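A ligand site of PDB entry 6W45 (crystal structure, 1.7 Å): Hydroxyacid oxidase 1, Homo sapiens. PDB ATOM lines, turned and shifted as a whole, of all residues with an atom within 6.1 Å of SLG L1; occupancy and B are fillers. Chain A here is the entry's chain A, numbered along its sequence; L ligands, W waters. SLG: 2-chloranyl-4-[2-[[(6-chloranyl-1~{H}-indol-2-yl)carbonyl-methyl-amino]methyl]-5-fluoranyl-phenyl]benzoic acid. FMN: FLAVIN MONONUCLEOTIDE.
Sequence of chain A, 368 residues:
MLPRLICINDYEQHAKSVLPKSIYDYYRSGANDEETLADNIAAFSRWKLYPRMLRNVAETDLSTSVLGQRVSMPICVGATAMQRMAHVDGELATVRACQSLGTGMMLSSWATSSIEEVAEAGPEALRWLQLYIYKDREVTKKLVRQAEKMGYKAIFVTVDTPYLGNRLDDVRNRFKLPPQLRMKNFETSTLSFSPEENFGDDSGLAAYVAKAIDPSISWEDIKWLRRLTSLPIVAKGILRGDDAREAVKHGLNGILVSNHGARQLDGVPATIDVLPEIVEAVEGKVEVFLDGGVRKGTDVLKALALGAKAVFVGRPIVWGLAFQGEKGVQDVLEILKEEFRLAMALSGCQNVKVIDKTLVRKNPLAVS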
ATOM      1  N   SER A  22       8.573  -8.493   4.995  1.00  0.00           N
ATOM      2  CA  SER A  22       8.802  -9.941   5.285  1.00  0.00           C
ATOM      3  C   SER A  22       9.758 -10.084   6.480  1.00  0.00           C
ATOM      4  O   SER A  22       9.499 -10.927   7.356  1.00  0.00           O
ATOM      5  CB  SER A  22       9.297 -10.675   4.058  1.00  0.00           C
ATOM      6  OG  SER A  22      10.540 -10.138   3.613  1.00  0.00           O
ATOM      7  N   ILE A  23      10.823  -9.261   6.518  1.00  0.00           N
ATOM      8  CA  ILE A  23      11.886  -9.297   7.562  1.00  0.00           C
ATOM      9  C   ILE A  23      11.308  -8.734   8.867  1.00  0.00           C
ATOM     10  O   ILE A  23      11.522  -9.375   9.910  1.00  0.00           O
ATOM     11  CB  ILE A  23      13.154  -8.550   7.109  1.00  0.00           C
ATOM     12  CG1 ILE A  23      13.810  -9.246   5.898  1.00  0.00           C
ATOM     13  CG2 ILE A  23      14.117  -8.413   8.258  1.00  0.00           C
ATOM     14  CD1 ILE A  23      15.118  -8.590   5.449  1.00  0.00           C
ATOM     15  N   TYR A  26       9.031 -11.354  10.188  1.00  0.00           N
ATOM     16  CA  TYR A  26       9.801 -12.516  10.701  1.00  0.00           C
ATOM     17  C   TYR A  26      10.216 -12.226  12.155  1.00  0.00           C
ATOM     18  O   TYR A  26      10.043 -13.090  13.073  1.00  0.00           O
ATOM     19  CB  TYR A  26      11.038 -12.834   9.868  1.00  0.00           C
ATOM     20  CG  TYR A  26      11.945 -13.828  10.553  1.00  0.00           C
ATOM     21  CD1 TYR A  26      11.536 -15.144  10.667  1.00  0.00           C
ATOM     22  CD2 TYR A  26      13.131 -13.464  11.153  1.00  0.00           C
ATOM     23  CE1 TYR A  26      12.311 -16.063  11.353  1.00  0.00           C
ATOM     24  CE2 TYR A  26      13.927 -14.371  11.834  1.00  0.00           C
ATOM     25  CZ  TYR A  26      13.475 -15.677  11.956  1.00  0.00           C
ATOM     26  OH  TYR A  26      14.206 -16.568  12.649  1.00  0.00           O
ATOM     27  N   ALA A  81      18.449 -15.101  16.287  1.00  0.00           N
ATOM     28  CA  ALA A  81      19.096 -15.603  15.050  1.00  0.00           C
ATOM     29  C   ALA A  81      19.261 -14.464  14.036  1.00  0.00           C
ATOM     30  O   ALA A  81      18.382 -13.586  13.953  1.00  0.00           O
ATOM     31  CB  ALA A  81      18.235 -16.685  14.485  1.00  0.00           C
ATOM     32  N   MET A  82      20.319 -14.566  13.242  1.00  0.00           N
ATOM     33  CA  MET A  82      20.460 -13.887  11.918  1.00  0.00           C
ATOM     34  C   MET A  82      20.289 -12.376  12.032  1.00  0.00           C
ATOM     35  O   MET A  82      19.512 -11.727  11.248  1.00  0.00           O
ATOM     36  CB  MET A  82      19.435 -14.448  10.933  1.00  0.00           C
ATOM     37  CG  MET A  82      19.638 -15.929  10.697  1.00  0.00           C
ATOM     38  SD  MET A  82      18.310 -16.549   9.667  1.00  0.00           S
ATOM     39  CE  MET A  82      16.877 -15.722  10.338  1.00  0.00           C
ATOM     40  N   MET A  85      20.472  -9.759   8.994  1.00  0.00           N
ATOM     41  CA  MET A  85      19.274  -9.344   8.230  1.00  0.00           C
ATOM     42  C   MET A  85      18.815  -7.945   8.661  1.00  0.00           C
ATOM     43  O   MET A  85      18.102  -7.314   7.898  1.00  0.00           O
ATOM     44  CB  MET A  85      18.098 -10.303   8.407  1.00  0.00           C
ATOM     45  CG  MET A  85      18.365 -11.702   7.950  1.00  0.00           C
ATOM     46  SD  MET A  85      16.748 -12.435   7.674  1.00  0.00           S
ATOM     47  CE  MET A  85      16.075 -12.290   9.343  1.00  0.00           C
ATOM     48  N   SER A 108      23.438 -16.375  19.648  1.00  0.00           N
ATOM     49  CA  SER A 108      22.538 -17.386  19.057  1.00  0.00           C
ATOM     50  C   SER A 108      23.350 -18.518  18.443  1.00  0.00           C
ATOM     51  O   SER A 108      24.435 -18.254  17.893  1.00  0.00           O
ATOM     52  CB  SER A 108      21.668 -16.812  17.956  1.00  0.00           C
ATOM     53  OG  SER A 108      21.045 -17.869  17.223  1.00  0.00           O
ATOM     54  N   TRP A 110      22.322 -19.753  15.766  1.00  0.00           N
ATOM     55  CA  TRP A 110      22.003 -19.519  14.332  1.00  0.00           C
ATOM     56  C   TRP A 110      22.504 -18.127  13.923  1.00  0.00           C
ATOM     57  O   TRP A 110      21.716 -17.373  13.280  1.00  0.00           O
ATOM     58  CB  TRP A 110      20.505 -19.651  14.085  1.00  0.00           C
ATOM     59  CG  TRP A 110      19.958 -20.986  14.448  1.00  0.00           C
ATOM     60  CD1 TRP A 110      19.173 -21.307  15.530  1.00  0.00           C
ATOM     61  CD2 TRP A 110      20.165 -22.210  13.724  1.00  0.00           C
ATOM     62  NE1 TRP A 110      18.884 -22.635  15.517  1.00  0.00           N
ATOM     63  CE2 TRP A 110      19.465 -23.219  14.419  1.00  0.00           C
ATOM     64  CE3 TRP A 110      20.845 -22.525  12.535  1.00  0.00           C
ATOM     65  CZ2 TRP A 110      19.445 -24.541  13.948  1.00  0.00           C
ATOM     66  CZ3 TRP A 110      20.818 -23.834  12.083  1.00  0.00           C
ATOM     67  CH2 TRP A 110      20.131 -24.818  12.792  1.00  0.00           C
ATOM     68  N   GLN A 130      24.452 -19.536  23.376  1.00  0.00           N
ATOM     69  CA  GLN A 130      23.200 -20.304  23.343  1.00  0.00           C
ATOM     70  C   GLN A 130      23.415 -21.479  22.393  1.00  0.00           C
ATOM     71  O   GLN A 130      23.872 -21.253  21.269  1.00  0.00           O
ATOM     72  CB  GLN A 130      22.027 -19.417  22.953  1.00  0.00           C
ATOM     73  CG  GLN A 130      20.760 -20.214  22.742  1.00  0.00           C
ATOM     74  CD  GLN A 130      20.567 -20.810  21.369  1.00  0.00           C
ATOM     75  OE1 GLN A 130      20.641 -20.117  20.356  1.00  0.00           O
ATOM     76  NE2 GLN A 130      20.196 -22.086  21.331  1.00  0.00           N
ATOM     77  N   TYR A 132      21.817 -25.505  21.031  1.00  0.00           N
ATOM     78  CA  TYR A 132      20.886 -26.630  20.918  1.00  0.00           C
ATOM     79  C   TYR A 132      21.708 -27.921  21.020  1.00  0.00           C
ATOM     80  O   TYR A 132      22.863 -27.938  20.537  1.00  0.00           O
ATOM     81  CB  TYR A 132      20.158 -26.559  19.581  1.00  0.00           C
ATOM     82  CG  TYR A 132      19.093 -25.490  19.534  1.00  0.00           C
ATOM     83  CD1 TYR A 132      17.908 -25.688  20.218  1.00  0.00           C
ATOM     84  CD2 TYR A 132      19.246 -24.305  18.836  1.00  0.00           C
ATOM     85  CE1 TYR A 132      16.919 -24.727  20.222  1.00  0.00           C
ATOM     86  CE2 TYR A 132      18.244 -23.349  18.791  1.00  0.00           C
ATOM     87  CZ  TYR A 132      17.081 -23.567  19.497  1.00  0.00           C
ATOM     88  OH  TYR A 132      16.087 -22.625  19.548  1.00  0.00           O
ATOM     89  N   THR A 158      18.973 -24.250  24.996  1.00  0.00           N
ATOM     90  CA  THR A 158      17.536 -24.035  24.704  1.00  0.00           C
ATOM     91  C   THR A 158      16.830 -25.389  24.693  1.00  0.00           C
ATOM     92  O   THR A 158      17.283 -26.314  23.935  1.00  0.00           O
ATOM     93  CB  THR A 158      17.354 -23.235  23.417  1.00  0.00           C
ATOM     94  OG1 THR A 158      18.089 -22.020  23.543  1.00  0.00           O
ATOM     95  CG2 THR A 158      15.874 -23.012  23.166  1.00  0.00           C
ATOM     96  N   THR A 161      12.431 -26.290  22.101  1.00  0.00           N
ATOM     97  CA  THR A 161      12.338 -26.363  20.620  1.00  0.00           C
ATOM     98  C   THR A 161      12.690 -27.756  20.128  1.00  0.00           C
ATOM     99  O   THR A 161      13.629 -27.910  19.344  1.00  0.00           O
ATOM    100  CB  THR A 161      13.175 -25.237  19.987  1.00  0.00           C
ATOM    101  OG1 THR A 161      12.797 -24.000  20.621  1.00  0.00           O
ATOM    102  CG2 THR A 161      12.927 -25.039  18.507  1.00  0.00           C
ATOM    103  N   LEU A 164      10.321 -26.655  15.513  1.00  0.00           N
ATOM    104  CA  LEU A 164       9.995 -25.220  15.381  1.00  0.00           C
ATOM    105  C   LEU A 164       8.476 -24.963  15.521  1.00  0.00           C
ATOM    106  O   LEU A 164       7.672 -25.634  14.856  1.00  0.00           O
ATOM    107  CB  LEU A 164      10.491 -24.700  14.033  1.00  0.00           C
ATOM    108  CG  LEU A 164      11.931 -24.190  14.003  1.00  0.00           C
ATOM    109  CD1 LEU A 164      12.084 -22.908  14.780  1.00  0.00           C
ATOM    110  CD2 LEU A 164      12.887 -25.219  14.538  1.00  0.00           C
ATOM    111  N   ARG A 167       4.751 -20.202  12.960  1.00  0.00           N
ATOM    112  CA  ARG A 167       4.417 -18.764  12.808  1.00  0.00           C
ATOM    113  C   ARG A 167       3.721 -18.631  11.435  1.00  0.00           C
ATOM    114  O   ARG A 167       4.345 -19.042  10.423  1.00  0.00           O
ATOM    115  CB  ARG A 167       5.687 -17.911  12.935  1.00  0.00           C
ATOM    116  CG  ARG A 167       6.492 -18.129  14.221  1.00  0.00           C
ATOM    117  CD  ARG A 167       7.822 -17.388  14.178  1.00  0.00           C
ATOM    118  NE  ARG A 167       8.563 -17.911  13.028  1.00  0.00           N
ATOM    119  CZ  ARG A 167       8.606 -17.362  11.795  1.00  0.00           C
ATOM    120  NH1 ARG A 167       9.289 -17.964  10.821  1.00  0.00           N
ATOM    121  NH2 ARG A 167       7.981 -16.222  11.529  1.00  0.00           N
ATOM    122  N   LEU A 205      13.116 -23.743   4.517  1.00  0.00           N
ATOM    123  CA  LEU A 205      14.114 -23.331   5.544  1.00  0.00           C
ATOM    124  C   LEU A 205      13.931 -24.193   6.799  1.00  0.00           C
ATOM    125  O   LEU A 205      14.940 -24.556   7.404  1.00  0.00           O
ATOM    126  CB  LEU A 205      13.932 -21.836   5.857  1.00  0.00           C
ATOM    127  CG  LEU A 205      14.119 -20.880   4.680  1.00  0.00           C
ATOM    128  CD1 LEU A 205      13.948 -19.436   5.124  1.00  0.00           C
ATOM    129  CD2 LEU A 205      15.472 -21.072   4.019  1.00  0.00           C
ATOM    130  N   ALA A 206      12.668 -24.494   7.161  1.00  0.00           N
ATOM    131  CA  ALA A 206      12.284 -25.309   8.348  1.00  0.00           C
ATOM    132  C   ALA A 206      12.769 -26.747   8.171  1.00  0.00           C
ATOM    133  O   ALA A 206      13.088 -27.379   9.191  1.00  0.00           O
ATOM    134  CB  ALA A 206      10.783 -25.252   8.567  1.00  0.00           C
ATOM    135  N   TYR A 208      15.545 -27.623   6.505  1.00  0.00           N
ATOM    136  CA  TYR A 208      16.993 -27.478   6.796  1.00  0.00           C
ATOM    137  C   TYR A 208      17.241 -27.527   8.315  1.00  0.00           C
ATOM    138  O   TYR A 208      18.171 -28.212   8.749  1.00  0.00           O
ATOM    139  CB  TYR A 208      17.574 -26.178   6.227  1.00  0.00           C
ATOM    140  CG  TYR A 208      18.983 -25.907   6.707  1.00  0.00           C
ATOM    141  CD1 TYR A 208      20.058 -26.610   6.190  1.00  0.00           C
ATOM    142  CD2 TYR A 208      19.227 -24.992   7.731  1.00  0.00           C
ATOM    143  CE1 TYR A 208      21.349 -26.392   6.656  1.00  0.00           C
ATOM    144  CE2 TYR A 208      20.510 -24.763   8.191  1.00  0.00           C
ATOM    145  CZ  TYR A 208      21.578 -25.463   7.654  1.00  0.00           C
ATOM    146  OH  TYR A 208      22.855 -25.248   8.095  1.00  0.00           O
ATOM    147  N   VAL A 209      16.436 -26.803   9.099  1.00  0.00           N
ATOM    148  CA  VAL A 209      16.592 -26.721  10.582  1.00  0.00           C
ATOM    149  C   VAL A 209      16.147 -28.035  11.230  1.00  0.00           C
ATOM    150  O   VAL A 209      16.737 -28.410  12.248  1.00  0.00           O
ATOM    151  CB  VAL A 209      15.806 -25.534  11.158  1.00  0.00           C
ATOM    152  CG1 VAL A 209      15.914 -25.480  12.673  1.00  0.00           C
ATOM    153  CG2 VAL A 209      16.265 -24.228  10.528  1.00  0.00           C
ATOM    154  N   ILE A 213      17.918 -29.853  14.453  1.00  0.00           N
ATOM    155  CA  ILE A 213      17.277 -29.864  15.800  1.00  0.00           C
ATOM    156  C   ILE A 213      16.769 -31.267  16.156  1.00  0.00           C
ATOM    157  O   ILE A 213      15.943 -31.803  15.397  1.00  0.00           O
ATOM    158  CB  ILE A 213      16.136 -28.832  15.770  1.00  0.00           C
ATOM    159  CG1 ILE A 213      16.674 -27.417  15.592  1.00  0.00           C
ATOM    160  CG2 ILE A 213      15.230 -28.956  16.981  1.00  0.00           C
ATOM    161  CD1 ILE A 213      17.350 -26.880  16.820  1.00  0.00           C
ATOM    162  N   HIS A 260      10.275 -18.435  24.626  1.00  0.00           N
ATOM    163  CA  HIS A 260      10.983 -18.325  23.311  1.00  0.00           C
ATOM    164  C   HIS A 260      10.378 -17.128  22.580  1.00  0.00           C
ATOM    165  O   HIS A 260      10.140 -17.221  21.336  1.00  0.00           O
ATOM    166  CB  HIS A 260      10.809 -19.621  22.515  1.00  0.00           C
ATOM    167  CG  HIS A 260      11.915 -19.883  21.547  1.00  0.00           C
ATOM    168  ND1 HIS A 260      12.790 -20.970  21.682  1.00  0.00           N
ATOM    169  CD2 HIS A 260      12.244 -19.242  20.389  1.00  0.00           C
ATOM    170  CE1 HIS A 260      13.627 -20.973  20.643  1.00  0.00           C
ATOM    171  NE2 HIS A 260      13.345 -19.877  19.841  1.00  0.00           N
ATOM    172  N   ARG A 263       7.157 -17.716  20.352  1.00  0.00           N
ATOM    173  CA  ARG A 263       7.356 -18.230  18.976  1.00  0.00           C
ATOM    174  C   ARG A 263       7.260 -19.765  18.940  1.00  0.00           C
ATOM    175  O   ARG A 263       7.395 -20.337  17.832  1.00  0.00           O
ATOM    176  CB  ARG A 263       8.722 -17.769  18.458  1.00  0.00           C
ATOM    177  CG  ARG A 263       8.796 -16.266  18.280  1.00  0.00           C
ATOM    178  CD  ARG A 263      10.202 -15.850  17.943  1.00  0.00           C
ATOM    179  NE  ARG A 263      10.631 -16.143  16.569  1.00  0.00           N
ATOM    180  CZ  ARG A 263      10.486 -15.325  15.522  1.00  0.00           C
ATOM    181  NH1 ARG A 263       9.796 -14.213  15.612  1.00  0.00           N
ATOM    182  NH2 ARG A 263      11.019 -15.663  14.348  1.00  0.00           N
ATOM    183  N   GLN A 264       7.010 -20.439  20.063  1.00  0.00           N
ATOM    184  CA  GLN A 264       7.033 -21.925  20.107  1.00  0.00           C
ATOM    185  C   GLN A 264       5.578 -22.386  20.305  1.00  0.00           C
ATOM    186  O   GLN A 264       4.785 -22.338  19.372  1.00  0.00           O
ATOM    187  CB  GLN A 264       8.045 -22.385  21.175  1.00  0.00           C
ATOM    188  CG  GLN A 264       9.485 -22.408  20.666  1.00  0.00           C
ATOM    189  CD  GLN A 264       9.656 -23.329  19.472  1.00  0.00           C
ATOM    190  OE1 GLN A 264       9.846 -22.862  18.336  1.00  0.00           O
ATOM    191  NE2 GLN A 264       9.466 -24.614  19.675  1.00  0.00           N
HETATM  192  C1  SLG L   1      14.211 -19.779  10.710  1.00  0.00           C
HETATM  193  C2  SLG L   1      15.624 -20.223  10.433  1.00  0.00           C
HETATM  194  C3  SLG L   1      16.065 -20.319   9.102  1.00  0.00           C
HETATM  195  C7  SLG L   1      16.509 -20.542  11.461  1.00  0.00           C
HETATM  196  C8  SLG L   1      16.133 -20.449  12.902  1.00  0.00           C
HETATM  197  C9  SLG L   1      15.826 -19.236  13.497  1.00  0.00           C
HETATM  198  C10 SLG L   1      15.556 -19.164  14.853  1.00  0.00           C
HETATM  199  C11 SLG L   1      15.557 -20.298  15.644  1.00  0.00           C
HETATM  200  C12 SLG L   1      15.278 -20.152  17.113  1.00  0.00           C
HETATM  201  C13 SLG L   1      15.814 -21.509  15.030  1.00  0.00           C
HETATM  202  C14 SLG L   1      16.113 -21.602  13.683  1.00  0.00           C
HETATM  203  C15 SLG L   1      12.547 -19.684   8.824  1.00  0.00           C
HETATM  204  C16 SLG L   1      12.922 -18.298   8.474  1.00  0.00           C
HETATM  205  C19 SLG L   1      14.485 -15.135   7.633  1.00  0.00           C
HETATM  206  C20 SLG L   1      13.901 -14.064   6.980  1.00  0.00           C
HETATM  207  C21 SLG L   1      12.584 -14.140   6.620  1.00  0.00           C
HETATM  208  C22 SLG L   1      11.806 -15.257   6.886  1.00  0.00           C
HETATM  209 CL1  SLG L   1      11.857 -12.795   5.794  1.00  0.00          CL
HETATM  210  C23 SLG L   1      12.418 -16.326   7.539  1.00  0.00           C
HETATM  211  C18 SLG L   1      13.759 -16.283   7.914  1.00  0.00           C
HETATM  212  C17 SLG L   1      14.062 -17.561   8.495  1.00  0.00           C
HETATM  213  N1  SLG L   1      11.916 -17.554   7.904  1.00  0.00           N
HETATM  214  O2  SLG L   1      11.596 -20.219   8.254  1.00  0.00           O
HETATM  215  N   SLG L   1      13.230 -20.366   9.801  1.00  0.00           N
HETATM  216  C   SLG L   1      12.997 -21.799   9.933  1.00  0.00           C
HETATM  217  C6  SLG L   1      17.800 -20.957  11.169  1.00  0.00           C
HETATM  218  C5  SLG L   1      18.184 -21.049   9.855  1.00  0.00           C
HETATM  219  F   SLG L   1      19.443 -21.517   9.581  1.00  0.00           F
HETATM  220  C4  SLG L   1      17.356 -20.735   8.811  1.00  0.00           C
HETATM  221 CL   SLG L   1      15.663 -22.996  15.912  1.00  0.00          CL
HETATM  222  O1  SLG L   1      15.967 -20.721  17.923  1.00  0.00           O
HETATM  223  O   SLG L   1      14.275 -19.398  17.390  1.00  0.00           O
HETATM  224  N1  FMN L   2      16.171 -18.291  21.032  1.00  0.00           N
HETATM  225  C2  FMN L   2      17.209 -19.133  20.968  1.00  0.00           C
HETATM  226  O2  FMN L   2      17.498 -19.867  21.977  1.00  0.00           O
HETATM  227  N3  FMN L   2      18.026 -19.180  19.846  1.00  0.00           N
HETATM  228  C4  FMN L   2      17.743 -18.435  18.774  1.00  0.00           C
HETATM  229  O4  FMN L   2      18.447 -18.480  17.727  1.00  0.00           O
HETATM  230  C4A FMN L   2      16.616 -17.529  18.809  1.00  0.00           C
HETATM  231  N5  FMN L   2      16.252 -16.725  17.728  1.00  0.00           N
HETATM  232  C5A FMN L   2      15.271 -15.875  17.840  1.00  0.00           C
HETATM  233  C6  FMN L   2      15.004 -15.037  16.764  1.00  0.00           C
HETATM  234  C7  FMN L   2      13.992 -14.139  16.847  1.00  0.00           C
HETATM  235  C7M FMN L   2      13.642 -13.206  15.701  1.00  0.00           C
HETATM  236  C8  FMN L   2      13.227 -13.965  18.063  1.00  0.00           C
HETATM  237  C8M FMN L   2      12.171 -12.912  18.145  1.00  0.00           C
HETATM  238  C9  FMN L   2      13.497 -14.731  19.170  1.00  0.00           C
HETATM  239  C9A FMN L   2      14.499 -15.713  19.061  1.00  0.00           C
HETATM  240  N10 FMN L   2      14.836 -16.543  20.129  1.00  0.00           N
HETATM  241  C10 FMN L   2      15.855 -17.437  20.024  1.00  0.00           C
HETATM  242  C1' FMN L   2      14.151 -16.404  21.425  1.00  0.00           C
HETATM  243  C2' FMN L   2      14.902 -15.341  22.214  1.00  0.00           C
HETATM  244  O2' FMN L   2      16.151 -15.839  22.742  1.00  0.00           O
HETATM  245  C3' FMN L   2      14.118 -14.764  23.408  1.00  0.00           C
HETATM  246  O3' FMN L   2      13.652 -15.908  24.212  1.00  0.00           O
HETATM  247  C4' FMN L   2      12.934 -13.942  23.074  1.00  0.00           C
HETATM  248  O4' FMN L   2      13.287 -13.034  21.978  1.00  0.00           O
HETATM  249  C5' FMN L   2      12.558 -13.037  24.268  1.00  0.00           C
HETATM  250  O5' FMN L   2      11.380 -12.312  24.074  1.00  0.00           O
HETATM  251  P   FMN L   2      11.390 -10.739  23.570  1.00  0.00           P
HETATM  252  O1P FMN L   2      12.423  -9.960  24.333  1.00  0.00           O
HETATM  253  O2P FMN L   2      11.715 -10.829  22.050  1.00  0.00           O
HETATM  254  O3P FMN L   2      10.000 -10.337  23.822  1.00  0.00           O
HETATM  255  O   HOH W   1      12.378 -18.312  13.671  1.00  0.00           O
HETATM  256  O   HOH W   2       8.998 -17.593   8.230  1.00  0.00           O
HETATM  257  O   HOH W   3      12.019 -18.702  16.277  1.00  0.00           O
HETATM  258  O   HOH W   4      10.787 -20.058  12.165  1.00  0.00           O
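OG of Ser 108 lies within hydrogen-bond range of O4 of FMN L2, 2.7 Å away. An oxygen (O1) of SLG L1 sits at hydrogen-bond distance from the side-chain hydroxyl (OH) of Tyr 132 (2.5 Å). The side-chain hydroxyl of Thr 158 sits at hydrogen-bond distance from an oxygen (O2) of FMN L2, at 2.7 Å. OE1 of Gln 130 lies within hydrogen-bond range of N3 of FMN L2 (2.8 Å). A nitrogen (N5) of FMN L2 is in hydrogen-bond range of the backbone NH of Ala 81. NE2 of His 260 lies within hydrogen-bond range of O of SLG L1 (2.7 Å). A nitrogen (N1) of FMN L2 sits at hydrogen-bond distance from a ring nitrogen (NE2) of His 260.
An oxygen (O1) of SLG L1 sits close to a nitrogen (N3) of FMN L2, at 3.2 Å.
The backbone carbonyl oxygen (O) of Trp 110 sits at hydrogen-bond distance from the backbone NH (N) of Met 82, at 3.1 Å. N of Trp 110 is in hydrogen-bond range of OG of Ser 108, at 2.7 Å. NH1 of Arg 263 is in hydrogen-bond range of O of Tyr 26 (2.8 Å). A ring nitrogen (ND1) of His 260 lies close to the side-chain hydroxyl (OG1) of Thr 161 (3.2 Å).
Ser 22 touches SLG L1 (O to CL1, 3.4 Å). Ile 23 touches SLG L1 (N to CL1, 3.8 Å). OH of Tyr 26 touches C9 of SLG L1, 3.2 Å away. CB of Ala 81 touches C9 of SLG L1, at 3.6 Å. Met 82 touches SLG L1. Met 85 touches SLG L1. Trp 110 touches SLG L1. CD1 of Leu 164 touches CL of SLG L1 (3.8 Å). Arg 167 touches SLG L1. Leu 205 touches SLG L1 (CD1 to C16, 3.7 Å). Ala 206 touches SLG L1 (N to C, 3.9 Å). CE2 of Tyr 208 touches F of SLG L1 (3.7 Å). CG2 of Val 209 touches C6 of SLG L1, at 3.7 Å. Hydrophobic or aromatic side chains within 4 Å of SLG L1: Tyr 26, Ala 81, Met 82, Met 85, Trp 110, Tyr 132, Leu 164, Leu 205, Tyr 208, Val 209 and His 260. The nearest printed residue that does not touch SLG L1 is Thr 161 (4.3 Å).
Water W3 lies within hydrogen-bond range of O of SLG L1 (2.6 Å) and NE of Arg 263 (2.9 Å). Water W2 lies within hydrogen-bond range of the guanidinium group of Arg 167 (2.6 Å) and a nitrogen (N1) of SLG L1 (2.9 Å). Water W1 lies within hydrogen-bond range of the side-chain hydroxyl of Tyr 26 and the guanidinium group of Arg 263.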
